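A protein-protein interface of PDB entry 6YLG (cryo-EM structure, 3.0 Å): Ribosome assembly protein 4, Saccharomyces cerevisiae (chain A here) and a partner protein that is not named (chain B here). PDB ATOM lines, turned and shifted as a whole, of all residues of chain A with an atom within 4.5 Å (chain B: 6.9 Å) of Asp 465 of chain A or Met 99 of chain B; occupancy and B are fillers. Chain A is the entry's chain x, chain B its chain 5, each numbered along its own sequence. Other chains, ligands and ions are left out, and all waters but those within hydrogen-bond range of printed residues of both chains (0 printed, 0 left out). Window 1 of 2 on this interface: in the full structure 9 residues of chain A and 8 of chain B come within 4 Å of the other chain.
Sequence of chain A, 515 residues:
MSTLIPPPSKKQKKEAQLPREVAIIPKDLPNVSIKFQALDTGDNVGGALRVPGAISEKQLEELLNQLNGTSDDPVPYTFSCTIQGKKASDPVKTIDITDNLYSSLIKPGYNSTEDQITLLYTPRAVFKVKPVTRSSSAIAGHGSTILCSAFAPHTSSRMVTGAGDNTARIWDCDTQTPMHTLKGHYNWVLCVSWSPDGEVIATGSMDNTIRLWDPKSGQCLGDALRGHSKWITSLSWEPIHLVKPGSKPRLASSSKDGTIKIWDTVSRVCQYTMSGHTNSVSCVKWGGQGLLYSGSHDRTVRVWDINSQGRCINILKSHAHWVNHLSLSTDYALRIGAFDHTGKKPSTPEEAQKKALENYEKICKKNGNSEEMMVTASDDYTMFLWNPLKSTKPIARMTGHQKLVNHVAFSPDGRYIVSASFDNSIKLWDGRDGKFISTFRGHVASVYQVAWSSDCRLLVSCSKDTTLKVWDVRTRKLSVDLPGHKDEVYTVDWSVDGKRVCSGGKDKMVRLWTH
NZ of Lys 102 of chain B lies within hydrogen-bond range of O of Val 444 of chain A, at 3.2 Å.
A ring nitrogen (ND1) of His 443 of chain A is in hydrogen-bond range of the side-chain carboxylate (OD2) of Asp 465 of chain A (2.7 Å). N of Val 444 of chain A sits at hydrogen-bond distance from OD2 of Asp 465 of chain A (3.5 Å). OG of Ser 463 of chain A sits at hydrogen-bond distance from OD2 of Asp 465 of chain A, 2.7 Å away. The side-chain carboxylate (OD1) of Asp 465 of chain A sits at hydrogen-bond distance from the side-chain hydroxyl (OG1) of Thr 467 of chain A (2.6 Å).
Among the printed residues, pairs that only touch across the chains: Val 444 of chain A with Met 99 of chain B (3.4 Å), Val 444 of chain A with Lys 103 of chain B (3.9 Å), Asp 465 of chain A with Met 99 of chain B (3.6 Å) and Asp 487 of chain A with Leu 95 of chain B (3.3 Å).
Of the printed residues of chain B, Val 444 of chain A touches Met 99, Lys 102 and Lys 103. Of the printed residues of chain B, Asp 487 of chain A touches Leu 95. Of the printed residues of chain A, Leu 95 of chain B touches Asp 487 (3.3 Å). Met 99 of chain B touches just these residues of chain A: Val 444 (3.4 Å) and Asp 465 (3.6 Å). Of the printed residues of chain A, Lys 102 of chain B touches Val 444. Of the printed residues of chain A, Lys 103 of chain B touches Val 444.
Of the 11 printed residues of chain B, 4 touch a printed residue of chain A. Hydrophobic or aromatic side chains of chain B within 4 Å of the printed part of chain A: Leu 95 and Met 99. Printed residues of chain A that touch a printed residue of chain B: Val 444, Asp 465 and Asp 487. Hydrophobic or aromatic side chains of chain A within 4 Å of the printed part of chain B: Val 444.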
ATOM      1  N   HIS A 443      20.630  -5.579  16.310  1.00  0.00           N
ATOM      2  CA  HIS A 443      19.316  -5.200  16.800  1.00  0.00           C
ATOM      3  C   HIS A 443      19.248  -3.696  17.025  1.00  0.00           C
ATOM      4  O   HIS A 443      20.270  -3.007  17.084  1.00  0.00           O
ATOM      5  CB  HIS A 443      18.995  -5.945  18.093  1.00  0.00           C
ATOM      6  CG  HIS A 443      18.355  -7.278  17.873  1.00  0.00           C
ATOM      7  ND1 HIS A 443      17.196  -7.434  17.144  1.00  0.00           N
ATOM      8  CD2 HIS A 443      18.712  -8.518  18.280  1.00  0.00           C
ATOM      9  CE1 HIS A 443      16.867  -8.712  17.112  1.00  0.00           C
ATOM     10  NE2 HIS A 443      17.770  -9.391  17.796  1.00  0.00           N
ATOM     11  N   VAL A 444      18.021  -3.193  17.148  1.00  0.00           N
ATOM     12  CA  VAL A 444      17.748  -1.766  17.250  1.00  0.00           C
ATOM     13  C   VAL A 444      16.853  -1.436  18.438  1.00  0.00           C
ATOM     14  O   VAL A 444      16.384  -0.300  18.556  1.00  0.00           O
ATOM     15  CB  VAL A 444      17.140  -1.229  15.944  1.00  0.00           C
ATOM     16  CG1 VAL A 444      18.223  -1.058  14.898  1.00  0.00           C
ATOM     17  CG2 VAL A 444      16.052  -2.161  15.439  1.00  0.00           C
ATOM     18  N   ALA A 445      16.606  -2.391  19.329  1.00  0.00           N
ATOM     19  CA  ALA A 445      15.760  -2.138  20.484  1.00  0.00           C
ATOM     20  C   ALA A 445      16.028  -3.216  21.526  1.00  0.00           C
ATOM     21  O   ALA A 445      16.937  -4.039  21.372  1.00  0.00           O
ATOM     22  CB  ALA A 445      14.289  -2.073  20.061  1.00  0.00           C
ATOM     23  N   SER A 463      13.826  -9.727  20.253  1.00  0.00           N
ATOM     24  CA  SER A 463      14.028  -8.333  20.616  1.00  0.00           C
ATOM     25  C   SER A 463      12.706  -7.586  20.650  1.00  0.00           C
ATOM     26  O   SER A 463      11.654  -8.103  20.267  1.00  0.00           O
ATOM     27  CB  SER A 463      14.990  -7.645  19.644  1.00  0.00           C
ATOM     28  OG  SER A 463      15.102  -6.262  19.929  1.00  0.00           O
ATOM     29  N   LYS A 464      12.789  -6.342  21.125  1.00  0.00           N
ATOM     30  CA  LYS A 464      11.645  -5.441  21.108  1.00  0.00           C
ATOM     31  C   LYS A 464      11.290  -5.043  19.687  1.00  0.00           C
ATOM     32  O   LYS A 464      10.123  -4.765  19.394  1.00  0.00           O
ATOM     33  CB  LYS A 464      11.955  -4.210  21.957  1.00  0.00           C
ATOM     34  CG  LYS A 464      10.879  -3.143  21.967  1.00  0.00           C
ATOM     35  CD  LYS A 464      11.141  -2.132  23.065  1.00  0.00           C
ATOM     36  CE  LYS A 464       9.981  -1.180  23.241  1.00  0.00           C
ATOM     37  NZ  LYS A 464      10.174  -0.313  24.430  1.00  0.00           N
ATOM     38  N   ASP A 465      12.277  -5.001  18.799  1.00  0.00           N
ATOM     39  CA  ASP A 465      11.984  -4.952  17.378  1.00  0.00           C
ATOM     40  C   ASP A 465      11.310  -6.253  16.962  1.00  0.00           C
ATOM     41  O   ASP A 465      11.351  -7.258  17.678  1.00  0.00           O
ATOM     42  CB  ASP A 465      13.259  -4.716  16.566  1.00  0.00           C
ATOM     43  CG  ASP A 465      14.314  -5.782  16.795  1.00  0.00           C
ATOM     44  OD1 ASP A 465      14.099  -6.946  16.400  1.00  0.00           O
ATOM     45  OD2 ASP A 465      15.369  -5.450  17.374  1.00  0.00           O
ATOM     46  N   THR A 466      10.696  -6.235  15.786  1.00  0.00           N
ATOM     47  CA  THR A 466       9.890  -7.371  15.356  1.00  0.00           C
ATOM     48  C   THR A 466      10.719  -8.522  14.805  1.00  0.00           C
ATOM     49  O   THR A 466      10.132  -9.494  14.323  1.00  0.00           O
ATOM     50  CB  THR A 466       8.884  -6.923  14.297  1.00  0.00           C
ATOM     51  OG1 THR A 466       9.568  -6.658  13.067  1.00  0.00           O
ATOM     52  CG2 THR A 466       8.155  -5.667  14.752  1.00  0.00           C
ATOM     53  N   THR A 467      12.042  -8.454  14.860  1.00  0.00           N
ATOM     54  CA  THR A 467      12.895  -9.438  14.217  1.00  0.00           C
ATOM     55  C   THR A 467      13.418 -10.458  15.219  1.00  0.00           C
ATOM     56  O   THR A 467      13.626 -10.164  16.398  1.00  0.00           O
ATOM     57  CB  THR A 467      14.080  -8.756  13.532  1.00  0.00           C
ATOM     58  OG1 THR A 467      15.065  -8.411  14.514  1.00  0.00           O
ATOM     59  CG2 THR A 467      13.627  -7.498  12.816  1.00  0.00           C
ATOM     60  N   ASP A 487       5.286  -6.909  15.717  1.00  0.00           N
ATOM     61  CA  ASP A 487       5.303  -6.233  17.008  1.00  0.00           C
ATOM     62  C   ASP A 487       6.386  -6.874  17.869  1.00  0.00           C
ATOM     63  O   ASP A 487       7.197  -7.672  17.386  1.00  0.00           O
ATOM     64  CB  ASP A 487       3.927  -6.294  17.678  1.00  0.00           C
ATOM     65  CG  ASP A 487       3.613  -5.046  18.470  1.00  0.00           C
ATOM     66  OD1 ASP A 487       4.538  -4.496  19.101  1.00  0.00           O
ATOM     67  OD2 ASP A 487       2.442  -4.613  18.460  1.00  0.00           O
ATOM     68  N   VAL A 489       8.496  -9.160  20.093  1.00  0.00           N
ATOM     69  CA  VAL A 489       8.607 -10.607  20.240  1.00  0.00           C
ATOM     70  C   VAL A 489       9.110 -10.903  21.643  1.00  0.00           C
ATOM     71  O   VAL A 489      10.238 -10.538  21.994  1.00  0.00           O
ATOM     72  CB  VAL A 489       9.550 -11.202  19.180  1.00  0.00           C
ATOM     73  CG1 VAL A 489       9.696 -12.699  19.379  1.00  0.00           C
ATOM     74  CG2 VAL A 489       9.038 -10.893  17.783  1.00  0.00           C
ATOM     75  N   ARG B  94       3.203   2.554  12.802  1.00  0.00           N
ATOM     76  CA  ARG B  94       4.092   3.461  13.519  1.00  0.00           C
ATOM     77  C   ARG B  94       5.328   2.742  14.041  1.00  0.00           C
ATOM     78  O   ARG B  94       6.421   3.315  14.046  1.00  0.00           O
ATOM     79  CB  ARG B  94       3.346   4.127  14.672  1.00  0.00           C
ATOM     80  CG  ARG B  94       2.275   5.102  14.228  1.00  0.00           C
ATOM     81  CD  ARG B  94       1.948   6.096  15.326  1.00  0.00           C
ATOM     82  NE  ARG B  94       1.778   5.444  16.623  1.00  0.00           N
ATOM     83  CZ  ARG B  94       0.651   4.879  17.058  1.00  0.00           C
ATOM     84  NH1 ARG B  94       0.623   4.321  18.259  1.00  0.00           N
ATOM     85  NH2 ARG B  94      -0.447   4.857  16.309  1.00  0.00           N
ATOM     86  N   LEU B  95       5.182   1.488  14.465  1.00  0.00           N
ATOM     87  CA  LEU B  95       6.325   0.747  14.983  1.00  0.00           C
ATOM     88  C   LEU B  95       7.325   0.430  13.880  1.00  0.00           C
ATOM     89  O   LEU B  95       8.542   0.562  14.078  1.00  0.00           O
ATOM     90  CB  LEU B  95       5.841  -0.537  15.655  1.00  0.00           C
ATOM     91  CG  LEU B  95       6.793  -1.226  16.630  1.00  0.00           C
ATOM     92  CD1 LEU B  95       7.077  -0.353  17.843  1.00  0.00           C
ATOM     93  CD2 LEU B  95       6.201  -2.552  17.048  1.00  0.00           C
ATOM     94  N   ALA B  96       6.839   0.000  12.713  1.00  0.00           N
ATOM     95  CA  ALA B  96       7.752  -0.220  11.599  1.00  0.00           C
ATOM     96  C   ALA B  96       8.435   1.070  11.164  1.00  0.00           C
ATOM     97  O   ALA B  96       9.633   1.050  10.847  1.00  0.00           O
ATOM     98  CB  ALA B  96       7.010  -0.841  10.417  1.00  0.00           C
ATOM     99  N   ALA B  97       7.712   2.192  11.170  1.00  0.00           N
ATOM    100  CA  ALA B  97       8.342   3.468  10.848  1.00  0.00           C
ATOM    101  C   ALA B  97       9.410   3.828  11.872  1.00  0.00           C
ATOM    102  O   ALA B  97      10.471   4.353  11.519  1.00  0.00           O
ATOM    103  CB  ALA B  97       7.287   4.569  10.770  1.00  0.00           C
ATOM    104  N   LYS B  98       9.144   3.547  13.149  1.00  0.00           N
ATOM    105  CA  LYS B  98      10.110   3.843  14.201  1.00  0.00           C
ATOM    106  C   LYS B  98      11.378   3.021  14.024  1.00  0.00           C
ATOM    107  O   LYS B  98      12.493   3.542  14.152  1.00  0.00           O
ATOM    108  CB  LYS B  98       9.474   3.574  15.563  1.00  0.00           C
ATOM    109  CG  LYS B  98      10.379   3.826  16.751  1.00  0.00           C
ATOM    110  CD  LYS B  98       9.553   4.115  17.989  1.00  0.00           C
ATOM    111  CE  LYS B  98      10.387   4.059  19.257  1.00  0.00           C
ATOM    112  NZ  LYS B  98      11.466   5.080  19.273  1.00  0.00           N
ATOM    113  N   MET B  99      11.228   1.732  13.721  1.00  0.00           N
ATOM    114  CA  MET B  99      12.391   0.891  13.479  1.00  0.00           C
ATOM    115  C   MET B  99      13.179   1.333  12.253  1.00  0.00           C
ATOM    116  O   MET B  99      14.416   1.334  12.293  1.00  0.00           O
ATOM    117  CB  MET B  99      11.969  -0.571  13.304  1.00  0.00           C
ATOM    118  CG  MET B  99      11.620  -1.340  14.587  1.00  0.00           C
ATOM    119  SD  MET B  99      12.790  -1.225  15.958  1.00  0.00           S
ATOM    120  CE  MET B  99      11.835  -0.260  17.122  1.00  0.00           C
ATOM    121  N   HIS B 100      12.497   1.709  11.171  1.00  0.00           N
ATOM    122  CA  HIS B 100      13.195   2.222   9.997  1.00  0.00           C
ATOM    123  C   HIS B 100      13.966   3.498  10.324  1.00  0.00           C
ATOM    124  O   HIS B 100      15.119   3.667   9.903  1.00  0.00           O
ATOM    125  CB  HIS B 100      12.196   2.476   8.870  1.00  0.00           C
ATOM    126  CG  HIS B 100      12.838   2.780   7.554  1.00  0.00           C
ATOM    127  ND1 HIS B 100      12.667   3.982   6.903  1.00  0.00           N
ATOM    128  CD2 HIS B 100      13.651   2.038   6.768  1.00  0.00           C
ATOM    129  CE1 HIS B 100      13.349   3.967   5.772  1.00  0.00           C
ATOM    130  NE2 HIS B 100      13.954   2.798   5.666  1.00  0.00           N
ATOM    131  N   ALA B 101      13.333   4.413  11.064  1.00  0.00           N
ATOM    132  CA  ALA B 101      14.007   5.639  11.472  1.00  0.00           C
ATOM    133  C   ALA B 101      15.237   5.340  12.313  1.00  0.00           C
ATOM    134  O   ALA B 101      16.284   5.975  12.133  1.00  0.00           O
ATOM    135  CB  ALA B 101      13.042   6.533  12.247  1.00  0.00           C
ATOM    136  N   LYS B 102      15.136   4.362  13.213  1.00  0.00           N
ATOM    137  CA  LYS B 102      16.276   4.008  14.051  1.00  0.00           C
ATOM    138  C   LYS B 102      17.402   3.423  13.211  1.00  0.00           C
ATOM    139  O   LYS B 102      18.582   3.721  13.432  1.00  0.00           O
ATOM    140  CB  LYS B 102      15.846   3.025  15.139  1.00  0.00           C
ATOM    141  CG  LYS B 102      15.725   3.661  16.507  1.00  0.00           C
ATOM    142  CD  LYS B 102      15.116   2.701  17.508  1.00  0.00           C
ATOM    143  CE  LYS B 102      15.058   3.309  18.895  1.00  0.00           C
ATOM    144  NZ  LYS B 102      15.201   2.275  19.951  1.00  0.00           N
ATOM    145  N   LYS B 103      17.053   2.596  12.224  1.00  0.00           N
ATOM    146  CA  LYS B 103      18.086   2.008  11.382  1.00  0.00           C
ATOM    147  C   LYS B 103      18.790   3.057  10.532  1.00  0.00           C
ATOM    148  O   LYS B 103      20.005   2.963  10.327  1.00  0.00           O
ATOM    149  CB  LYS B 103      17.498   0.920  10.486  1.00  0.00           C
ATOM    150  CG  LYS B 103      17.495  -0.456  11.132  1.00  0.00           C
ATOM    151  CD  LYS B 103      17.164  -1.567  10.146  1.00  0.00           C
ATOM    152  CE  LYS B 103      18.027  -2.793  10.412  1.00  0.00           C
ATOM    153  NZ  LYS B 103      17.566  -4.000   9.673  1.00  0.00           N
ATOM    154  N   VAL B 104      18.062   4.058  10.032  1.00  0.00           N
ATOM    155  CA  VAL B 104      18.732   5.069   9.217  1.00  0.00           C
ATOM    156  C   VAL B 104      19.564   6.007  10.087  1.00  0.00           C
ATOM    157  O   VAL B 104      20.658   6.418   9.686  1.00  0.00           O
ATOM    158  CB  VAL B 104      17.739   5.848   8.328  1.00  0.00           C
ATOM    159  CG1 VAL B 104      17.025   4.903   7.382  1.00  0.00           C
ATOM    160  CG2 VAL B 104      16.743   6.630   9.141  1.00  0.00           C
